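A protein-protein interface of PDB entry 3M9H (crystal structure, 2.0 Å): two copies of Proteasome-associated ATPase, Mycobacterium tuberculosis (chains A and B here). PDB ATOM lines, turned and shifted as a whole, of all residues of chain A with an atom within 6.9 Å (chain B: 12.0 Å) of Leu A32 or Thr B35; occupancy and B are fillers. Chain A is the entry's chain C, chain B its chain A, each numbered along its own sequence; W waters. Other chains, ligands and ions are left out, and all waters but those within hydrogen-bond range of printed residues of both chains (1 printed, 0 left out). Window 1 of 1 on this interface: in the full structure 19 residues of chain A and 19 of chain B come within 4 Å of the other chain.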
ATOM      1  N   LEU A  25      21.352 -25.884  36.744  1.00  0.00           N
ATOM      2  CA  LEU A  25      21.074 -24.614  36.086  1.00  0.00           C
ATOM      3  C   LEU A  25      21.877 -24.537  34.785  1.00  0.00           C
ATOM      4  O   LEU A  25      21.402 -23.963  33.786  1.00  0.00           O
ATOM      5  CB  LEU A  25      21.496 -23.485  37.038  1.00  0.00           C
ATOM      6  CG  LEU A  25      20.427 -23.238  38.111  1.00  0.00           C
ATOM      7  CD1 LEU A  25      20.950 -22.357  39.223  1.00  0.00           C
ATOM      8  CD2 LEU A  25      19.229 -22.547  37.452  1.00  0.00           C
ATOM      9  N   ALA A  27      22.744 -27.043  32.877  1.00  0.00           N
ATOM     10  CA  ALA A  27      22.061 -27.927  31.903  1.00  0.00           C
ATOM     11  C   ALA A  27      20.830 -27.249  31.297  1.00  0.00           C
ATOM     12  O   ALA A  27      20.538 -27.423  30.088  1.00  0.00           O
ATOM     13  CB  ALA A  27      21.666 -29.323  32.548  1.00  0.00           C
ATOM     14  N   ARG A  28      20.063 -26.540  32.134  1.00  0.00           N
ATOM     15  CA  ARG A  28      18.897 -25.827  31.599  1.00  0.00           C
ATOM     16  C   ARG A  28      19.370 -24.700  30.685  1.00  0.00           C
ATOM     17  O   ARG A  28      18.730 -24.461  29.672  1.00  0.00           O
ATOM     18  CB  ARG A  28      17.997 -25.276  32.704  1.00  0.00           C
ATOM     19  CG  ARG A  28      17.325 -26.434  33.402  1.00  0.00           C
ATOM     20  CD  ARG A  28      16.331 -25.990  34.503  1.00  0.00           C
ATOM     21  NE  ARG A  28      15.410 -27.100  34.783  1.00  0.00           N
ATOM     22  CZ  ARG A  28      15.576 -28.039  35.728  1.00  0.00           C
ATOM     23  NH1 ARG A  28      16.662 -28.045  36.501  1.00  0.00           N
ATOM     24  NH2 ARG A  28      14.656 -28.990  35.900  1.00  0.00           N
ATOM     25  N   ASN A  29      20.425 -23.965  31.073  1.00  0.00           N
ATOM     26  CA  ASN A  29      21.005 -22.995  30.153  1.00  0.00           C
ATOM     27  C   ASN A  29      21.340 -23.549  28.751  1.00  0.00           C
ATOM     28  O   ASN A  29      21.013 -22.897  27.736  1.00  0.00           O
ATOM     29  CB  ASN A  29      22.142 -22.194  30.834  1.00  0.00           C
ATOM     30  CG  ASN A  29      22.909 -21.266  29.865  1.00  0.00           C
ATOM     31  OD1 ASN A  29      23.777 -21.722  29.088  1.00  0.00           O
ATOM     32  ND2 ASN A  29      22.646 -19.945  29.954  1.00  0.00           N
ATOM     33  N   SER A  30      21.986 -24.720  28.683  1.00  0.00           N
ATOM     34  CA  SER A  30      22.255 -25.394  27.404  1.00  0.00           C
ATOM     35  C   SER A  30      20.973 -25.782  26.667  1.00  0.00           C
ATOM     36  O   SER A  30      20.857 -25.613  25.435  1.00  0.00           O
ATOM     37  CB  SER A  30      23.044 -26.679  27.638  1.00  0.00           C
ATOM     38  OG  SER A  30      24.369 -26.298  27.794  1.00  0.00           O
ATOM     39  N   LYS A  31      20.032 -26.340  27.389  1.00  0.00           N
ATOM     40  CA  LYS A  31      18.734 -26.640  26.764  1.00  0.00           C
ATOM     41  C   LYS A  31      18.071 -25.387  26.127  1.00  0.00           C
ATOM     42  O   LYS A  31      17.518 -25.444  24.990  1.00  0.00           O
ATOM     43  CB  LYS A  31      17.768 -27.297  27.843  1.00  0.00           C
ATOM     44  CG  LYS A  31      16.401 -27.717  27.267  1.00  0.00           C
ATOM     45  CD  LYS A  31      15.563 -28.497  28.277  1.00  0.00           C
ATOM     46  CE  LYS A  31      14.296 -28.941  27.690  1.00  0.00           C
ATOM     47  NZ  LYS A  31      13.546 -29.756  28.814  1.00  0.00           N
ATOM     48  N   LEU A  32      18.062 -24.284  26.865  1.00  0.00           N
ATOM     49  CA  LEU A  32      17.550 -23.010  26.316  1.00  0.00           C
ATOM     50  C   LEU A  32      18.314 -22.574  25.072  1.00  0.00           C
ATOM     51  O   LEU A  32      17.676 -22.232  24.012  1.00  0.00           O
ATOM     52  CB  LEU A  32      17.592 -21.912  27.386  1.00  0.00           C
ATOM     53  CG  LEU A  32      16.669 -22.137  28.581  1.00  0.00           C
ATOM     54  CD1 LEU A  32      17.088 -21.223  29.678  1.00  0.00           C
ATOM     55  CD2 LEU A  32      15.190 -21.782  28.169  1.00  0.00           C
ATOM     56  N   MET A  33      19.661 -22.612  25.135  1.00  0.00           N
ATOM     57  CA  MET A  33      20.422 -22.169  23.944  1.00  0.00           C
ATOM     58  C   MET A  33      20.161 -23.072  22.731  1.00  0.00           C
ATOM     59  O   MET A  33      20.117 -22.565  21.595  1.00  0.00           O
ATOM     60  CB  MET A  33      21.923 -22.213  24.209  1.00  0.00           C
ATOM     61  CG  MET A  33      22.756 -21.372  23.176  1.00  0.00           C
ATOM     62  SD  MET A  33      23.041 -19.830  24.048  1.00  0.00           S
ATOM     63  CE  MET A  33      24.024 -20.400  25.491  1.00  0.00           C
ATOM     64  N   GLU A  34      20.120 -24.406  22.914  1.00  0.00           N
ATOM     65  CA  GLU A  34      19.869 -25.287  21.718  1.00  0.00           C
ATOM     66  C   GLU A  34      18.465 -25.037  21.144  1.00  0.00           C
ATOM     67  O   GLU A  34      18.277 -24.991  19.930  1.00  0.00           O
ATOM     68  CB  GLU A  34      19.962 -26.784  22.082  1.00  0.00           C
ATOM     69  CG  GLU A  34      21.350 -27.297  22.026  1.00  0.00           C
ATOM     70  CD  GLU A  34      22.025 -27.182  20.663  1.00  0.00           C
ATOM     71  OE1 GLU A  34      21.381 -27.218  19.578  1.00  0.00           O
ATOM     72  OE2 GLU A  34      23.254 -27.083  20.697  1.00  0.00           O
ATOM     73  N   THR A  35      17.476 -24.913  22.026  1.00  0.00           N
ATOM     74  CA  THR A  35      16.106 -24.592  21.587  1.00  0.00           C
ATOM     75  C   THR A  35      16.082 -23.269  20.866  1.00  0.00           C
ATOM     76  O   THR A  35      15.377 -23.149  19.841  1.00  0.00           O
ATOM     77  CB  THR A  35      15.124 -24.518  22.758  1.00  0.00           C
ATOM     78  OG1 THR A  35      15.145 -25.761  23.464  1.00  0.00           O
ATOM     79  CG2 THR A  35      13.672 -24.301  22.281  1.00  0.00           C
ATOM     80  N   LEU A  36      16.770 -22.254  21.381  1.00  0.00           N
ATOM     81  CA  LEU A  36      16.800 -20.956  20.669  1.00  0.00           C
ATOM     82  C   LEU A  36      17.480 -21.033  19.312  1.00  0.00           C
ATOM     83  O   LEU A  36      17.052 -20.351  18.362  1.00  0.00           O
ATOM     84  CB  LEU A  36      17.495 -19.863  21.465  1.00  0.00           C
ATOM     85  CG  LEU A  36      16.791 -19.056  22.497  1.00  0.00           C
ATOM     86  CD1 LEU A  36      17.877 -18.096  23.116  1.00  0.00           C
ATOM     87  CD2 LEU A  36      15.582 -18.276  21.866  1.00  0.00           C
ATOM     88  N   LYS A  37      18.538 -21.833  19.208  1.00  0.00           N
ATOM     89  CA  LYS A  37      19.204 -22.047  17.913  1.00  0.00           C
ATOM     90  C   LYS A  37      18.273 -22.658  16.858  1.00  0.00           C
ATOM     91  O   LYS A  37      18.310 -22.270  15.697  1.00  0.00           O
ATOM     92  CB  LYS A  37      20.510 -22.830  18.097  1.00  0.00           C
ATOM     93  CG  LYS A  37      21.653 -21.890  18.658  1.00  0.00           C
ATOM     94  CD  LYS A  37      22.928 -22.626  19.169  1.00  0.00           C
ATOM     95  CE  LYS A  37      24.076 -21.566  19.647  1.00  0.00           C
ATOM     96  NZ  LYS A  37      25.414 -22.088  20.288  1.00  0.00           N
ATOM     97  N   LEU B  25       7.343 -22.588  15.720  1.00  0.00           N
ATOM     98  CA  LEU B  25       7.999 -21.535  16.484  1.00  0.00           C
ATOM     99  C   LEU B  25       7.253 -21.318  17.807  1.00  0.00           C
ATOM    100  O   LEU B  25       7.878 -21.091  18.855  1.00  0.00           O
ATOM    101  CB  LEU B  25       7.983 -20.242  15.658  1.00  0.00           C
ATOM    102  CG  LEU B  25       9.049 -20.305  14.582  1.00  0.00           C
ATOM    103  CD1 LEU B  25       8.802 -19.212  13.619  1.00  0.00           C
ATOM    104  CD2 LEU B  25      10.368 -20.066  15.303  1.00  0.00           C
ATOM    105  N   ALA B  26       5.915 -21.338  17.762  1.00  0.00           N
ATOM    106  CA  ALA B  26       5.163 -21.123  19.003  1.00  0.00           C
ATOM    107  C   ALA B  26       5.405 -22.270  19.991  1.00  0.00           C
ATOM    108  O   ALA B  26       5.533 -22.032  21.214  1.00  0.00           O
ATOM    109  CB  ALA B  26       3.644 -20.932  18.686  1.00  0.00           C
ATOM    110  N   ALA B  27       5.562 -23.502  19.498  1.00  0.00           N
ATOM    111  CA  ALA B  27       5.838 -24.637  20.396  1.00  0.00           C
ATOM    112  C   ALA B  27       7.229 -24.492  21.041  1.00  0.00           C
ATOM    113  O   ALA B  27       7.439 -24.872  22.238  1.00  0.00           O
ATOM    114  CB  ALA B  27       5.695 -26.017  19.623  1.00  0.00           C
ATOM    115  N   ARG B  28       8.197 -23.988  20.262  1.00  0.00           N
ATOM    116  CA  ARG B  28       9.551 -23.742  20.812  1.00  0.00           C
ATOM    117  C   ARG B  28       9.496 -22.610  21.800  1.00  0.00           C
ATOM    118  O   ARG B  28      10.155 -22.684  22.850  1.00  0.00           O
ATOM    119  CB  ARG B  28      10.586 -23.419  19.736  1.00  0.00           C
ATOM    120  CG  ARG B  28      10.829 -24.664  18.902  1.00  0.00           C
ATOM    121  CD  ARG B  28      12.041 -24.512  17.934  1.00  0.00           C
ATOM    122  NE  ARG B  28      12.392 -25.868  17.505  1.00  0.00           N
ATOM    123  CZ  ARG B  28      11.937 -26.451  16.395  1.00  0.00           C
ATOM    124  NH1 ARG B  28      11.116 -25.780  15.587  1.00  0.00           N
ATOM    125  NH2 ARG B  28      12.308 -27.693  16.088  1.00  0.00           N
ATOM    126  N   ASN B  29       8.751 -21.546  21.464  1.00  0.00           N
ATOM    127  CA  ASN B  29       8.497 -20.542  22.492  1.00  0.00           C
ATOM    128  C   ASN B  29       7.974 -21.093  23.837  1.00  0.00           C
ATOM    129  O   ASN B  29       8.496 -20.674  24.870  1.00  0.00           O
ATOM    130  CB  ASN B  29       7.658 -19.379  21.926  1.00  0.00           C
ATOM    131  CG  ASN B  29       7.314 -18.308  22.965  1.00  0.00           C
ATOM    132  OD1 ASN B  29       6.308 -18.432  23.719  1.00  0.00           O
ATOM    133  ND2 ASN B  29       8.090 -17.209  22.973  1.00  0.00           N
ATOM    134  N   SER B  30       6.978 -21.996  23.844  1.00  0.00           N
ATOM    135  CA  SER B  30       6.450 -22.567  25.078  1.00  0.00           C
ATOM    136  C   SER B  30       7.518 -23.421  25.760  1.00  0.00           C
ATOM    137  O   SER B  30       7.644 -23.389  26.991  1.00  0.00           O
ATOM    138  CB  SER B  30       5.254 -23.480  24.791  1.00  0.00           C
ATOM    139  OG  SER B  30       4.122 -22.640  24.746  1.00  0.00           O
ATOM    140  N   LYS B  31       8.274 -24.175  24.985  1.00  0.00           N
ATOM    141  CA  LYS B  31       9.366 -24.987  25.538  1.00  0.00           C
ATOM    142  C   LYS B  31      10.399 -24.097  26.279  1.00  0.00           C
ATOM    143  O   LYS B  31      10.864 -24.438  27.408  1.00  0.00           O
ATOM    144  CB  LYS B  31      10.075 -25.809  24.382  1.00  0.00           C
ATOM    145  CG  LYS B  31      11.257 -26.619  24.890  1.00  0.00           C
ATOM    146  CD  LYS B  31      11.856 -27.503  23.815  1.00  0.00           C
ATOM    147  CE  LYS B  31      12.785 -28.500  24.405  1.00  0.00           C
ATOM    148  NZ  LYS B  31      13.196 -29.454  23.257  1.00  0.00           N
ATOM    149  N   LEU B  32      10.760 -22.974  25.659  1.00  0.00           N
ATOM    150  CA  LEU B  32      11.685 -21.983  26.303  1.00  0.00           C
ATOM    151  C   LEU B  32      11.113 -21.444  27.590  1.00  0.00           C
ATOM    152  O   LEU B  32      11.826 -21.421  28.635  1.00  0.00           O
ATOM    153  CB  LEU B  32      11.999 -20.839  25.345  1.00  0.00           C
ATOM    154  CG  LEU B  32      12.859 -21.236  24.154  1.00  0.00           C
ATOM    155  CD1 LEU B  32      12.785 -20.168  23.201  1.00  0.00           C
ATOM    156  CD2 LEU B  32      14.360 -21.410  24.581  1.00  0.00           C
ATOM    157  N   MET B  33       9.822 -21.015  27.556  1.00  0.00           N
ATOM    158  CA  MET B  33       9.233 -20.444  28.775  1.00  0.00           C
ATOM    159  C   MET B  33       9.176 -21.482  29.899  1.00  0.00           C
ATOM    160  O   MET B  33       9.385 -21.107  31.065  1.00  0.00           O
ATOM    161  CB  MET B  33       7.807 -19.931  28.489  1.00  0.00           C
ATOM    162  CG  MET B  33       7.151 -19.224  29.650  1.00  0.00           C
ATOM    163  SD  MET B  33       7.810 -17.585  29.527  1.00  0.00           S
ATOM    164  CE  MET B  33       6.941 -17.095  27.954  1.00  0.00           C
ATOM    165  N   GLU B  34       8.809 -22.744  29.592  1.00  0.00           N
ATOM    166  CA  GLU B  34       8.700 -23.739  30.668  1.00  0.00           C
ATOM    167  C   GLU B  34      10.094 -23.959  31.287  1.00  0.00           C
ATOM    168  O   GLU B  34      10.239 -24.094  32.514  1.00  0.00           O
ATOM    169  CB  GLU B  34       8.201 -25.122  30.141  1.00  0.00           C
ATOM    170  CG  GLU B  34       6.836 -25.486  30.441  1.00  0.00           C
ATOM    171  CD  GLU B  34       6.425 -25.305  31.870  1.00  0.00           C
ATOM    172  OE1 GLU B  34       6.751 -26.126  32.773  1.00  0.00           O
ATOM    173  OE2 GLU B  34       5.715 -24.335  32.078  1.00  0.00           O
ATOM    174  N   THR B  35      11.096 -24.062  30.429  1.00  0.00           N
ATOM    175  CA  THR B  35      12.471 -24.333  30.883  1.00  0.00           C
ATOM    176  C   THR B  35      12.942 -23.150  31.717  1.00  0.00           C
ATOM    177  O   THR B  35      13.640 -23.348  32.739  1.00  0.00           O
ATOM    178  CB  THR B  35      13.445 -24.544  29.682  1.00  0.00           C
ATOM    179  OG1 THR B  35      12.972 -25.614  28.876  1.00  0.00           O
ATOM    180  CG2 THR B  35      14.842 -24.885  30.146  1.00  0.00           C
ATOM    181  N   LEU B  36      12.642 -21.923  31.281  1.00  0.00           N
ATOM    182  CA  LEU B  36      13.005 -20.738  32.066  1.00  0.00           C
ATOM    183  C   LEU B  36      12.322 -20.664  33.424  1.00  0.00           C
ATOM    184  O   LEU B  36      12.940 -20.236  34.416  1.00  0.00           O
ATOM    185  CB  LEU B  36      12.700 -19.430  31.348  1.00  0.00           C
ATOM    186  CG  LEU B  36      13.652 -18.869  30.325  1.00  0.00           C
ATOM    187  CD1 LEU B  36      12.966 -17.603  29.771  1.00  0.00           C
ATOM    188  CD2 LEU B  36      15.071 -18.530  30.937  1.00  0.00           C
ATOM    189  N   LYS B  37      11.054 -21.045  33.481  1.00  0.00           N
ATOM    190  CA  LYS B  37      10.327 -21.105  34.766  1.00  0.00           C
ATOM    191  C   LYS B  37      10.970 -22.099  35.758  1.00  0.00           C
ATOM    192  O   LYS B  37      11.070 -21.837  36.966  1.00  0.00           O
ATOM    193  CB  LYS B  37       8.811 -21.348  34.538  1.00  0.00           C
ATOM    194  CG  LYS B  37       8.042 -20.014  34.131  1.00  0.00           C
ATOM    195  CD  LYS B  37       6.555 -20.227  33.566  1.00  0.00           C
ATOM    196  CE  LYS B  37       5.889 -18.851  33.085  1.00  0.00           C
ATOM    197  NZ  LYS B  37       4.485 -18.862  32.376  1.00  0.00           N
ATOM    198  N   GLU B  38      11.440 -23.230  35.263  1.00  0.00           N
ATOM    199  CA  GLU B  38      12.205 -24.144  36.106  1.00  0.00           C
ATOM    200  C   GLU B  38      13.546 -23.581  36.580  1.00  0.00           C
ATOM    201  O   GLU B  38      13.920 -23.821  37.719  1.00  0.00           O
ATOM    202  CB  GLU B  38      12.537 -25.445  35.363  1.00  0.00           C
ATOM    203  CG  GLU B  38      11.343 -26.198  34.832  1.00  0.00           C
ATOM    204  CD  GLU B  38      11.803 -27.446  34.025  1.00  0.00           C
ATOM    205  OE1 GLU B  38      12.838 -27.375  33.291  1.00  0.00           O
ATOM    206  OE2 GLU B  38      11.148 -28.505  34.146  1.00  0.00           O
ATOM    207  N   ALA B  39      14.272 -22.868  35.710  1.00  0.00           N
ATOM    208  CA  ALA B  39      15.518 -22.219  36.071  1.00  0.00           C
ATOM    209  C   ALA B  39      15.294 -21.167  37.171  1.00  0.00           C
ATOM    210  O   ALA B  39      16.070 -21.093  38.111  1.00  0.00           O
ATOM    211  CB  ALA B  39      16.212 -21.579  34.797  1.00  0.00           C
ATOM    212  N   ARG B  40      14.230 -20.367  37.065  1.00  0.00           N
ATOM    213  CA  ARG B  40      13.895 -19.401  38.095  1.00  0.00           C
ATOM    214  C   ARG B  40      13.685 -20.064  39.484  1.00  0.00           C
ATOM    215  O   ARG B  40      14.158 -19.529  40.500  1.00  0.00           O
ATOM    216  CB  ARG B  40      12.607 -18.623  37.765  1.00  0.00           C
ATOM    217  CG  ARG B  40      12.251 -17.584  38.859  1.00  0.00           C
ATOM    218  CD  ARG B  40      10.699 -17.426  39.011  1.00  0.00           C
ATOM    219  NE  ARG B  40      10.173 -16.829  37.815  1.00  0.00           N
ATOM    220  CZ  ARG B  40       8.910 -16.866  37.368  1.00  0.00           C
ATOM    221  NH1 ARG B  40       7.941 -17.530  37.989  1.00  0.00           N
ATOM    222  NH2 ARG B  40       8.630 -16.236  36.238  1.00  0.00           N
ATOM    223  N   GLN B  41      12.914 -21.163  39.520  1.00  0.00           N
ATOM    224  CA  GLN B  41      12.686 -21.878  40.762  1.00  0.00           C
ATOM    225  C   GLN B  41      14.016 -22.388  41.368  1.00  0.00           C
ATOM    226  O   GLN B  41      14.243 -22.293  42.586  1.00  0.00           O
ATOM    227  CB  GLN B  41      11.775 -23.065  40.507  1.00  0.00           C
ATOM    228  CG  GLN B  41      10.360 -22.605  40.122  1.00  0.00           C
ATOM    229  CD  GLN B  41       9.457 -23.768  39.786  1.00  0.00           C
ATOM    230  OE1 GLN B  41       9.904 -24.760  39.202  1.00  0.00           O
ATOM    231  NE2 GLN B  41       8.180 -23.653  40.139  1.00  0.00           N
ATOM    232  N   GLN B  42      14.879 -22.937  40.523  1.00  0.00           N
ATOM    233  CA  GLN B  42      16.160 -23.454  41.001  1.00  0.00           C
ATOM    234  C   GLN B  42      17.125 -22.381  41.456  1.00  0.00           C
ATOM    235  O   GLN B  42      17.910 -22.612  42.378  1.00  0.00           O
ATOM    236  CB  GLN B  42      16.845 -24.182  39.875  1.00  0.00           C
ATOM    237  CG  GLN B  42      16.044 -25.334  39.357  1.00  0.00           C
ATOM    238  CD  GLN B  42      16.817 -26.509  39.559  1.00  0.00           C
ATOM    239  OE1 GLN B  42      17.157 -27.193  38.614  1.00  0.00           O
ATOM    240  NE2 GLN B  42      17.236 -26.720  40.794  1.00  0.00           N
ATOM    241  N   LEU B  43      17.137 -21.240  40.759  1.00  0.00           N
ATOM    242  CA  LEU B  43      17.916 -20.070  41.213  1.00  0.00           C
ATOM    243  C   LEU B  43      17.446 -19.560  42.551  1.00  0.00           C
ATOM    244  O   LEU B  43      18.275 -19.236  43.418  1.00  0.00           O
ATOM    245  CB  LEU B  43      17.838 -18.903  40.234  1.00  0.00           C
ATOM    246  CG  LEU B  43      18.690 -18.953  38.973  1.00  0.00           C
ATOM    247  CD1 LEU B  43      18.131 -17.871  38.017  1.00  0.00           C
ATOM    248  CD2 LEU B  43      20.209 -18.761  39.182  1.00  0.00           C
ATOM    249  N   LEU B  44      16.123 -19.525  42.737  1.00  0.00           N
ATOM    250  CA  LEU B  44      15.580 -19.148  44.054  1.00  0.00           C
ATOM    251  C   LEU B  44      16.001 -20.101  45.164  1.00  0.00           C
ATOM    252  O   LEU B  44      16.371 -19.675  46.229  1.00  0.00           O
ATOM    253  CB  LEU B  44      14.062 -19.001  43.999  1.00  0.00           C
ATOM    254  CG  LEU B  44      13.697 -17.768  43.133  1.00  0.00           C
ATOM    255  CD1 LEU B  44      12.176 -17.723  42.907  1.00  0.00           C
ATOM    256  CD2 LEU B  44      14.227 -16.345  43.689  1.00  0.00           C
HETATM  257  O   HOH W   1      14.072 -28.954  31.693  1.00  0.00           O
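The side-chain carboxylate of Glu B38 lies within salt-bridge range of the guanidinium group of Arg A28 (3.0 Å).
The guanidinium group (NH1) of Arg A28 lies close to the side-chain amide oxygen (OE1) of Gln B42 (2.3 Å).
The backbone carbonyl oxygen of Lys B31 is in hydrogen-bond range of the side-chain hydroxyl of Thr B35.
O of Lys A31 is in hydrogen-bond range of OG1 of Thr A35.
CD2 of Leu A25 touches O of Ala B39, 3.5 Å away.
Leu B43 touches Leu A25.
CD of Arg A28 touches N of Ala B39, at 3.9 Å.
Lys B31 touches Lys A31.
Lys A31 touches Thr B35 (CE to OG1, 3.8 Å).
Leu A32 touches Leu B32 (CD2 to O, 3.4 Å).
Leu A32 touches Thr B35 (CD2 to CB, 3.6 Å).
Leu A32 touches Leu B36 (CD1 to CD2, 3.6 Å).
O of Arg B28 touches CG2 of Thr A35, 3.9 Å away.
Thr A35 touches Leu B32.
Leu A32 touches just these residues of chain B: Leu B32, Thr B35 and Leu B36.
Thr B35 touches just these residues of chain A: Arg A28 (3.9 Å), Lys A31 (3.8 Å) and Leu A32 (3.6 Å).
No residue of chain B comes within 4 Å of Asn A29.
No residue of chain B comes within 4 Å of Ser A30.
No residue of chain B comes within 4 Å of Met A33.
Of chain B, only Arg B28 (3.9 Å), Lys B31 (3.7 Å) and Leu B32 (3.7 Å) come within 4 Å of Thr A35.
Of the printed residues of chain A, Glu B38 touches Arg A28 (3.0 Å).
Printed residues of chain A within 4 Å of Leu B43: Leu A25 (3.7 Å).
Printed residues of chain A within 4 Å of Lys B31: Lys A31 and Thr A35.
Of the printed residues of chain A, Ala B39 touches Leu A25 and Arg A28.
The nearest residue of chain B that does not touch Leu A32 is Lys B31 (5.1 Å).
The nearest residue of chain A that does not touch Thr B35 is Asn A29 (5.7 Å).
The nearest printed residue of chain A that does not touch Leu B36 is Arg A28 (6.4 Å).
Printed residues of chain B that touch a printed residue of chain A: Arg B28, Lys B31, Leu B32, Thr B35, Leu B36, Glu B38, Ala B39, Gln B42 and Leu B43.
Hydrophobic or aromatic side chains of chain B within 4 Å of the printed part of chain A: Leu B32, Leu B36 and Leu B43.
Of the 12 printed residues of chain A, 6 touch a printed residue of chain B.
Hydrophobic or aromatic side chains of chain A within 4 Å of the printed part of chain B: Leu A25, Leu A32 and Leu A36.
Among the printed residues, Asp or Glu carboxylates within 4 Å of a Lys or Arg side-chain nitrogen of the other chain: Arg A28 with Glu B38 (3.0 Å).
Arg A28 touches Thr B35, and with the chains exchanged Thr A35 touches Arg B28.
Lys B31 touches its own counterpart, Lys A31.
Leu B32 touches its own counterpart, Leu A32.
Leu A32 touches Thr B35, and with the chains exchanged Thr A35 touches Leu B32.
Positions printed for both chains: 25, 27, 28, 29, 30, 31, 32, 33, 34, 35, 36 and 37.
Of the 16 pairs that touch across the chains among the printed residues, 10 have their exchanged pair printed and touching as well.
Water W1 bridges the side-chain carboxylate of Glu B38 (2.6 Å) and the side-chain amino group of Lys A31 (3.0 Å).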
